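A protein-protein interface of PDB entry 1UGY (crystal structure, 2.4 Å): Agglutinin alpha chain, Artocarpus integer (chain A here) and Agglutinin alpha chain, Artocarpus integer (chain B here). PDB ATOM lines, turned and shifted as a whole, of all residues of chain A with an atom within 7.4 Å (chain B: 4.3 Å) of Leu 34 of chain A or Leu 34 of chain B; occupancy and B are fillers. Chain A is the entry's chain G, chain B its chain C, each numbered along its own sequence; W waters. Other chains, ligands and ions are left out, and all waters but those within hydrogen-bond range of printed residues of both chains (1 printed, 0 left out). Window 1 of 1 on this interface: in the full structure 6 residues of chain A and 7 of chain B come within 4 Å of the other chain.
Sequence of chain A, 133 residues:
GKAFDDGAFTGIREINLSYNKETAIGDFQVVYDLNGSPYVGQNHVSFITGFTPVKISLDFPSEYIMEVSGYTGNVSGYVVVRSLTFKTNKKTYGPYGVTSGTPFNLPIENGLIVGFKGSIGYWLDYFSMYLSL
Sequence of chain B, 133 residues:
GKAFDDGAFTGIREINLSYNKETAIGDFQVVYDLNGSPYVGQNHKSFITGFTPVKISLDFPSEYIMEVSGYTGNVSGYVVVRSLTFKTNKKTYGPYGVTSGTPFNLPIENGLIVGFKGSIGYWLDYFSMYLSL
Of the printed residues of chain B, Ala 8 of chain A touches Asn 35 (3.1 Å). Pro 38 of chain A touches none of the printed residues of chain B. Of the printed residues of chain A, Leu 34 of chain B touches Leu 34 (3.6 Å). Printed residues of chain A within 4 Å of Asn 35 of chain B: Asp 6, Gly 7, Ala 8 and Phe 9. The nearest printed residue of chain B that does not touch Gly 7 of chain A is Thr 10 of chain B (7.0 Å).
OD2 of Asp 6 of chain A sits at hydrogen-bond distance from OH of Tyr 32 of chain A. OG1 of Thr 10 of chain A lies within hydrogen-bond range of N of Asn 35 of chain A (3.0 Å). N of Asn 35 of chain B lies within hydrogen-bond range of OG1 of Thr 10 of chain B (3.1 Å). The backbone NH of Tyr 39 of chain B sits at hydrogen-bond distance from the backbone carbonyl oxygen of Tyr 32 of chain B, at 2.8 Å.
Asp 6 of chain A touches Asn 35 of chain B. Gly 7 of chain A touches Asn 35 of chain B. Asn 35 of chain B touches Phe 9 of chain A (OD1 to CZ, 3.7 Å). Leu 34 of chain B touches Leu 34 of chain A. Leu 34 of chain A touches Tyr 39 of chain B. Phe 9 of chain B touches Asn 35 of chain A (CZ to OD1, 3.7 Å).
The side-chain amide nitrogen (ND2) of Asn 35 of chain B sits close to the backbone NH (N) of Ala 8 of chain A, 3.1 Å away.
Of the 18 printed residues of chain A, 6 touch a printed residue of chain B. Printed residues of chain A that touch a printed residue of chain B: Asp 6, Gly 7, Ala 8, Phe 9, Leu 34 and Asn 35. Hydrophobic or aromatic side chains of chain A that line the printed part of chain B: Phe 9 and Leu 34. Of the 9 printed residues of chain B, 4 touch a printed residue of chain A. Printed residues of chain B that touch a printed residue of chain A: Phe 9, Leu 34, Asn 35 and Tyr 39. Hydrophobic or aromatic side chains of chain B within 4 Å of the printed part of chain A: Phe 9, Leu 34 and Tyr 39. Among the printed residues, 7 pairs touch across the chains.
Water W1 lies within hydrogen-bond range of OG1 of Thr 10 of chain B (2.8 Å) and O of Ala 8 of chain A (3.4 Å).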
ATOM      1  N   ASP A   6      14.807  33.089 -27.214  1.00  0.00           N
ATOM      2  CA  ASP A   6      15.387  31.762 -27.012  1.00  0.00           C
ATOM      3  C   ASP A   6      15.615  31.012 -28.322  1.00  0.00           C
ATOM      4  O   ASP A   6      16.537  30.210 -28.426  1.00  0.00           O
ATOM      5  CB  ASP A   6      14.487  30.902 -26.117  1.00  0.00           C
ATOM      6  CG  ASP A   6      14.633  31.227 -24.650  1.00  0.00           C
ATOM      7  OD1 ASP A   6      15.540  32.009 -24.294  1.00  0.00           O
ATOM      8  OD2 ASP A   6      13.848  30.685 -23.848  1.00  0.00           O
ATOM      9  N   GLY A   7      14.764  31.263 -29.311  1.00  0.00           N
ATOM     10  CA  GLY A   7      14.901  30.578 -30.582  1.00  0.00           C
ATOM     11  C   GLY A   7      14.019  29.343 -30.603  1.00  0.00           C
ATOM     12  O   GLY A   7      13.241  29.124 -29.673  1.00  0.00           O
ATOM     13  N   ALA A   8      14.149  28.528 -31.648  1.00  0.00           N
ATOM     14  CA  ALA A   8      13.340  27.320 -31.781  1.00  0.00           C
ATOM     15  C   ALA A   8      14.109  26.049 -31.408  1.00  0.00           C
ATOM     16  O   ALA A   8      15.296  25.938 -31.687  1.00  0.00           O
ATOM     17  CB  ALA A   8      12.810  27.211 -33.210  1.00  0.00           C
ATOM     18  N   PHE A   9      13.427  25.099 -30.772  1.00  0.00           N
ATOM     19  CA  PHE A   9      14.046  23.836 -30.379  1.00  0.00           C
ATOM     20  C   PHE A   9      13.250  22.616 -30.820  1.00  0.00           C
ATOM     21  O   PHE A   9      12.384  22.709 -31.687  1.00  0.00           O
ATOM     22  CB  PHE A   9      14.260  23.793 -28.870  1.00  0.00           C
ATOM     23  CG  PHE A   9      15.283  24.770 -28.390  1.00  0.00           C
ATOM     24  CD1 PHE A   9      14.941  26.099 -28.164  1.00  0.00           C
ATOM     25  CD2 PHE A   9      16.611  24.377 -28.226  1.00  0.00           C
ATOM     26  CE1 PHE A   9      15.904  27.023 -27.788  1.00  0.00           C
ATOM     27  CE2 PHE A   9      17.585  25.294 -27.851  1.00  0.00           C
ATOM     28  CZ  PHE A   9      17.234  26.617 -27.632  1.00  0.00           C
ATOM     29  N   THR A  10      13.554  21.471 -30.219  1.00  0.00           N
ATOM     30  CA  THR A  10      12.896  20.214 -30.562  1.00  0.00           C
ATOM     31  C   THR A  10      11.673  19.928 -29.705  1.00  0.00           C
ATOM     32  O   THR A  10      10.830  19.111 -30.074  1.00  0.00           O
ATOM     33  CB  THR A  10      13.868  19.029 -30.418  1.00  0.00           C
ATOM     34  OG1 THR A  10      15.035  19.273 -31.209  1.00  0.00           O
ATOM     35  CG2 THR A  10      13.219  17.749 -30.895  1.00  0.00           C
ATOM     36  N   GLY A  11      11.588  20.592 -28.557  1.00  0.00           N
ATOM     37  CA  GLY A  11      10.461  20.389 -27.669  1.00  0.00           C
ATOM     38  C   GLY A  11      10.656  21.109 -26.351  1.00  0.00           C
ATOM     39  O   GLY A  11      11.590  21.892 -26.199  1.00  0.00           O
ATOM     40  N   ILE A  12       9.778  20.846 -25.392  1.00  0.00           N
ATOM     41  CA  ILE A  12       9.872  21.483 -24.090  1.00  0.00           C
ATOM     42  C   ILE A  12       9.839  20.435 -22.988  1.00  0.00           C
ATOM     43  O   ILE A  12       8.956  19.579 -22.961  1.00  0.00           O
ATOM     44  CB  ILE A  12       8.727  22.488 -23.898  1.00  0.00           C
ATOM     45  CG1 ILE A  12       8.909  23.649 -24.877  1.00  0.00           C
ATOM     46  CG2 ILE A  12       8.692  22.973 -22.462  1.00  0.00           C
ATOM     47  CD1 ILE A  12       7.738  24.588 -24.943  1.00  0.00           C
ATOM     48  N   ARG A  13      10.814  20.508 -22.086  1.00  0.00           N
ATOM     49  CA  ARG A  13      10.924  19.560 -20.985  1.00  0.00           C
ATOM     50  C   ARG A  13      10.469  20.120 -19.644  1.00  0.00           C
ATOM     51  O   ARG A  13       9.876  19.407 -18.838  1.00  0.00           O
ATOM     52  CB  ARG A  13      12.369  19.075 -20.856  1.00  0.00           C
ATOM     53  CG  ARG A  13      12.794  18.094 -21.935  1.00  0.00           C
ATOM     54  CD  ARG A  13      14.268  17.745 -21.827  1.00  0.00           C
ATOM     55  NE  ARG A  13      14.643  16.709 -22.787  1.00  0.00           N
ATOM     56  CZ  ARG A  13      14.679  15.405 -22.518  1.00  0.00           C
ATOM     57  NH1 ARG A  13      14.371  14.962 -21.302  1.00  0.00           N
ATOM     58  NH2 ARG A  13      15.008  14.541 -23.469  1.00  0.00           N
ATOM     59  N   VAL A  31      13.526  24.828 -20.046  1.00  0.00           N
ATOM     60  CA  VAL A  31      14.478  23.760 -20.310  1.00  0.00           C
ATOM     61  C   VAL A  31      13.876  23.042 -21.515  1.00  0.00           C
ATOM     62  O   VAL A  31      12.858  22.351 -21.409  1.00  0.00           O
ATOM     63  CB  VAL A  31      14.602  22.769 -19.140  1.00  0.00           C
ATOM     64  CG1 VAL A  31      15.503  21.605 -19.547  1.00  0.00           C
ATOM     65  CG2 VAL A  31      15.163  23.474 -17.916  1.00  0.00           C
ATOM     66  N   TYR A  32      14.497  23.232 -22.670  1.00  0.00           N
ATOM     67  CA  TYR A  32      14.010  22.624 -23.897  1.00  0.00           C
ATOM     68  C   TYR A  32      14.620  21.262 -24.140  1.00  0.00           C
ATOM     69  O   TYR A  32      15.437  20.766 -23.364  1.00  0.00           O
ATOM     70  CB  TYR A  32      14.365  23.497 -25.115  1.00  0.00           C
ATOM     71  CG  TYR A  32      13.854  24.910 -25.062  1.00  0.00           C
ATOM     72  CD1 TYR A  32      14.613  25.926 -24.488  1.00  0.00           C
ATOM     73  CD2 TYR A  32      12.599  25.231 -25.573  1.00  0.00           C
ATOM     74  CE1 TYR A  32      14.129  27.239 -24.425  1.00  0.00           C
ATOM     75  CE2 TYR A  32      12.109  26.532 -25.514  1.00  0.00           C
ATOM     76  CZ  TYR A  32      12.875  27.529 -24.940  1.00  0.00           C
ATOM     77  OH  TYR A  32      12.384  28.810 -24.892  1.00  0.00           O
ATOM     78  N   ASP A  33      14.195  20.653 -25.233  1.00  0.00           N
ATOM     79  CA  ASP A  33      14.783  19.407 -25.641  1.00  0.00           C
ATOM     80  C   ASP A  33      15.475  19.745 -26.958  1.00  0.00           C
ATOM     81  O   ASP A  33      14.919  20.465 -27.794  1.00  0.00           O
ATOM     82  CB  ASP A  33      13.749  18.321 -25.897  1.00  0.00           C
ATOM     83  CG  ASP A  33      14.398  17.034 -26.355  1.00  0.00           C
ATOM     84  OD1 ASP A  33      15.185  16.465 -25.574  1.00  0.00           O
ATOM     85  OD2 ASP A  33      14.148  16.600 -27.497  1.00  0.00           O
ATOM     86  N   LEU A  34      16.699  19.262 -27.123  1.00  0.00           N
ATOM     87  CA  LEU A  34      17.426  19.488 -28.355  1.00  0.00           C
ATOM     88  C   LEU A  34      17.835  18.125 -28.883  1.00  0.00           C
ATOM     89  O   LEU A  34      18.834  17.550 -28.457  1.00  0.00           O
ATOM     90  CB  LEU A  34      18.663  20.366 -28.120  1.00  0.00           C
ATOM     91  CG  LEU A  34      19.503  20.687 -29.371  1.00  0.00           C
ATOM     92  CD1 LEU A  34      18.623  21.334 -30.437  1.00  0.00           C
ATOM     93  CD2 LEU A  34      20.651  21.611 -29.003  1.00  0.00           C
ATOM     94  N   ASN A  35      17.029  17.592 -29.787  1.00  0.00           N
ATOM     95  CA  ASN A  35      17.318  16.300 -30.382  1.00  0.00           C
ATOM     96  C   ASN A  35      17.568  15.202 -29.351  1.00  0.00           C
ATOM     97  O   ASN A  35      18.522  14.439 -29.458  1.00  0.00           O
ATOM     98  CB  ASN A  35      18.511  16.442 -31.330  1.00  0.00           C
ATOM     99  CG  ASN A  35      18.277  17.513 -32.385  1.00  0.00           C
ATOM    100  OD1 ASN A  35      19.103  18.409 -32.581  1.00  0.00           O
ATOM    101  ND2 ASN A  35      17.142  17.429 -33.064  1.00  0.00           N
ATOM    102  N   GLY A  36      16.701  15.135 -28.346  1.00  0.00           N
ATOM    103  CA  GLY A  36      16.820  14.097 -27.341  1.00  0.00           C
ATOM    104  C   GLY A  36      17.604  14.437 -26.101  1.00  0.00           C
ATOM    105  O   GLY A  36      17.571  13.685 -25.131  1.00  0.00           O
ATOM    106  N   SER A  37      18.311  15.563 -26.123  1.00  0.00           N
ATOM    107  CA  SER A  37      19.101  15.990 -24.973  1.00  0.00           C
ATOM    108  C   SER A  37      18.540  17.275 -24.351  1.00  0.00           C
ATOM    109  O   SER A  37      18.141  18.200 -25.061  1.00  0.00           O
ATOM    110  CB  SER A  37      20.556  16.214 -25.390  1.00  0.00           C
ATOM    111  OG  SER A  37      21.330  16.687 -24.300  1.00  0.00           O
ATOM    112  N   PRO A  38      18.499  17.343 -23.010  1.00  0.00           N
ATOM    113  CA  PRO A  38      17.975  18.547 -22.356  1.00  0.00           C
ATOM    114  C   PRO A  38      18.857  19.745 -22.667  1.00  0.00           C
ATOM    115  O   PRO A  38      20.081  19.643 -22.663  1.00  0.00           O
ATOM    116  CB  PRO A  38      18.019  18.188 -20.869  1.00  0.00           C
ATOM    117  CG  PRO A  38      17.931  16.692 -20.863  1.00  0.00           C
ATOM    118  CD  PRO A  38      18.829  16.312 -22.013  1.00  0.00           C
ATOM    119  N   TYR A  39      18.238  20.878 -22.946  1.00  0.00           N
ATOM    120  CA  TYR A  39      18.999  22.078 -23.225  1.00  0.00           C
ATOM    121  C   TYR A  39      18.437  23.173 -22.342  1.00  0.00           C
ATOM    122  O   TYR A  39      17.281  23.567 -22.479  1.00  0.00           O
ATOM    123  CB  TYR A  39      18.895  22.458 -24.701  1.00  0.00           C
ATOM    124  CG  TYR A  39      19.804  23.598 -25.081  1.00  0.00           C
ATOM    125  CD1 TYR A  39      19.399  24.920 -24.918  1.00  0.00           C
ATOM    126  CD2 TYR A  39      21.087  23.356 -25.575  1.00  0.00           C
ATOM    127  CE1 TYR A  39      20.245  25.979 -25.234  1.00  0.00           C
ATOM    128  CE2 TYR A  39      21.945  24.404 -25.896  1.00  0.00           C
ATOM    129  CZ  TYR A  39      21.518  25.715 -25.723  1.00  0.00           C
ATOM    130  OH  TYR A  39      22.362  26.762 -26.024  1.00  0.00           O
ATOM    131  N   PHE A  60       8.102  14.539 -20.544  1.00  0.00           N
ATOM    132  CA  PHE A  60       8.522  14.524 -21.949  1.00  0.00           C
ATOM    133  C   PHE A  60       8.943  13.110 -22.334  1.00  0.00           C
ATOM    134  O   PHE A  60       9.634  12.446 -21.570  1.00  0.00           O
ATOM    135  CB  PHE A  60       9.706  15.489 -22.131  1.00  0.00           C
ATOM    136  CG  PHE A  60      10.238  15.561 -23.539  1.00  0.00           C
ATOM    137  CD1 PHE A  60       9.640  16.385 -24.483  1.00  0.00           C
ATOM    138  CD2 PHE A  60      11.350  14.814 -23.917  1.00  0.00           C
ATOM    139  CE1 PHE A  60      10.141  16.467 -25.781  1.00  0.00           C
ATOM    140  CE2 PHE A  60      11.856  14.890 -25.210  1.00  0.00           C
ATOM    141  CZ  PHE A  60      11.245  15.722 -26.144  1.00  0.00           C
ATOM    142  N   PHE B   9      18.880  21.334 -36.750  1.00  0.00           N
ATOM    143  CA  PHE B   9      19.339  22.608 -36.229  1.00  0.00           C
ATOM    144  C   PHE B   9      18.808  23.779 -37.045  1.00  0.00           C
ATOM    145  O   PHE B   9      17.819  23.642 -37.759  1.00  0.00           O
ATOM    146  CB  PHE B   9      20.869  22.625 -36.178  1.00  0.00           C
ATOM    147  CG  PHE B   9      21.446  21.633 -35.208  1.00  0.00           C
ATOM    148  CD1 PHE B   9      21.578  20.293 -35.559  1.00  0.00           C
ATOM    149  CD2 PHE B   9      21.819  22.030 -33.926  1.00  0.00           C
ATOM    150  CE1 PHE B   9      22.074  19.363 -34.646  1.00  0.00           C
ATOM    151  CE2 PHE B   9      22.316  21.111 -33.006  1.00  0.00           C
ATOM    152  CZ  PHE B   9      22.442  19.775 -33.366  1.00  0.00           C
ATOM    153  N   THR B  10      19.469  24.929 -36.940  1.00  0.00           N
ATOM    154  CA  THR B  10      19.040  26.131 -37.646  1.00  0.00           C
ATOM    155  C   THR B  10      19.786  26.364 -38.948  1.00  0.00           C
ATOM    156  O   THR B  10      19.312  27.099 -39.812  1.00  0.00           O
ATOM    157  CB  THR B  10      19.217  27.373 -36.754  1.00  0.00           C
ATOM    158  OG1 THR B  10      18.503  27.177 -35.533  1.00  0.00           O
ATOM    159  CG2 THR B  10      18.676  28.616 -37.440  1.00  0.00           C
ATOM    160  N   TYR B  32      27.087  23.154 -36.561  1.00  0.00           N
ATOM    161  CA  TYR B  32      25.798  23.730 -36.910  1.00  0.00           C
ATOM    162  C   TYR B  32      25.601  25.101 -36.304  1.00  0.00           C
ATOM    163  O   TYR B  32      26.430  25.602 -35.536  1.00  0.00           O
ATOM    164  CB  TYR B  32      24.654  22.852 -36.403  1.00  0.00           C
ATOM    165  CG  TYR B  32      24.653  21.430 -36.908  1.00  0.00           C
ATOM    166  CD1 TYR B  32      25.307  20.421 -36.205  1.00  0.00           C
ATOM    167  CD2 TYR B  32      23.989  21.088 -38.085  1.00  0.00           C
ATOM    168  CE1 TYR B  32      25.296  19.099 -36.662  1.00  0.00           C
ATOM    169  CE2 TYR B  32      23.975  19.770 -38.548  1.00  0.00           C
ATOM    170  CZ  TYR B  32      24.629  18.786 -37.830  1.00  0.00           C
ATOM    171  OH  TYR B  32      24.618  17.485 -38.274  1.00  0.00           O
ATOM    172  N   ASP B  33      24.487  25.713 -36.665  1.00  0.00           N
ATOM    173  CA  ASP B  33      24.135  26.989 -36.092  1.00  0.00           C
ATOM    174  C   ASP B  33      22.881  26.706 -35.296  1.00  0.00           C
ATOM    175  O   ASP B  33      21.961  26.067 -35.798  1.00  0.00           O
ATOM    176  CB  ASP B  33      23.796  28.028 -37.150  1.00  0.00           C
ATOM    177  CG  ASP B  33      23.354  29.327 -36.528  1.00  0.00           C
ATOM    178  OD1 ASP B  33      24.222  30.069 -36.034  1.00  0.00           O
ATOM    179  OD2 ASP B  33      22.139  29.592 -36.502  1.00  0.00           O
ATOM    180  N   LEU B  34      22.847  27.158 -34.054  1.00  0.00           N
ATOM    181  CA  LEU B  34      21.673  26.953 -33.224  1.00  0.00           C
ATOM    182  C   LEU B  34      21.152  28.310 -32.806  1.00  0.00           C
ATOM    183  O   LEU B  34      21.663  28.920 -31.870  1.00  0.00           O
ATOM    184  CB  LEU B  34      22.018  26.127 -31.988  1.00  0.00           C
ATOM    185  CG  LEU B  34      20.820  25.771 -31.109  1.00  0.00           C
ATOM    186  CD1 LEU B  34      19.873  24.865 -31.871  1.00  0.00           C
ATOM    187  CD2 LEU B  34      21.306  25.083 -29.857  1.00  0.00           C
ATOM    188  N   ASN B  35      20.147  28.785 -33.529  1.00  0.00           N
ATOM    189  CA  ASN B  35      19.520  30.072 -33.254  1.00  0.00           C
ATOM    190  C   ASN B  35      20.512  31.220 -33.178  1.00  0.00           C
ATOM    191  O   ASN B  35      20.359  32.114 -32.351  1.00  0.00           O
ATOM    192  CB  ASN B  35      18.728  29.991 -31.952  1.00  0.00           C
ATOM    193  CG  ASN B  35      17.721  28.871 -31.966  1.00  0.00           C
ATOM    194  OD1 ASN B  35      17.664  28.058 -31.042  1.00  0.00           O
ATOM    195  ND2 ASN B  35      16.917  28.815 -33.018  1.00  0.00           N
ATOM    196  N   GLY B  36      21.528  31.199 -34.035  1.00  0.00           N
ATOM    197  CA  GLY B  36      22.500  32.273 -34.022  1.00  0.00           C
ATOM    198  C   GLY B  36      23.820  31.964 -33.338  1.00  0.00           C
ATOM    199  O   GLY B  36      24.754  32.756 -33.412  1.00  0.00           O
ATOM    200  N   SER B  37      23.912  30.827 -32.663  1.00  0.00           N
ATOM    201  CA  SER B  37      25.159  30.455 -32.004  1.00  0.00           C
ATOM    202  C   SER B  37      25.743  29.190 -32.621  1.00  0.00           C
ATOM    203  O   SER B  37      25.012  28.312 -33.078  1.00  0.00           O
ATOM    204  CB  SER B  37      24.929  30.217 -30.512  1.00  0.00           C
ATOM    205  OG  SER B  37      24.487  31.399 -29.867  1.00  0.00           O
ATOM    206  N   TYR B  39      27.213  25.557 -32.813  1.00  0.00           N
ATOM    207  CA  TYR B  39      27.005  24.385 -31.975  1.00  0.00           C
ATOM    208  C   TYR B  39      27.810  23.258 -32.597  1.00  0.00           C
ATOM    209  O   TYR B  39      27.544  22.836 -33.720  1.00  0.00           O
ATOM    210  CB  TYR B  39      25.520  24.019 -31.900  1.00  0.00           C
ATOM    211  CG  TYR B  39      25.231  22.925 -30.890  1.00  0.00           C
ATOM    212  CD1 TYR B  39      25.422  21.582 -31.211  1.00  0.00           C
ATOM    213  CD2 TYR B  39      24.786  23.237 -29.604  1.00  0.00           C
ATOM    214  CE1 TYR B  39      25.179  20.578 -30.281  1.00  0.00           C
ATOM    215  CE2 TYR B  39      24.540  22.235 -28.663  1.00  0.00           C
ATOM    216  CZ  TYR B  39      24.738  20.909 -29.010  1.00  0.00           C
ATOM    217  OH  TYR B  39      24.488  19.911 -28.091  1.00  0.00           O
HETATM  218  O   HOH W   1      16.319  25.484 -34.885  1.00  0.00           O
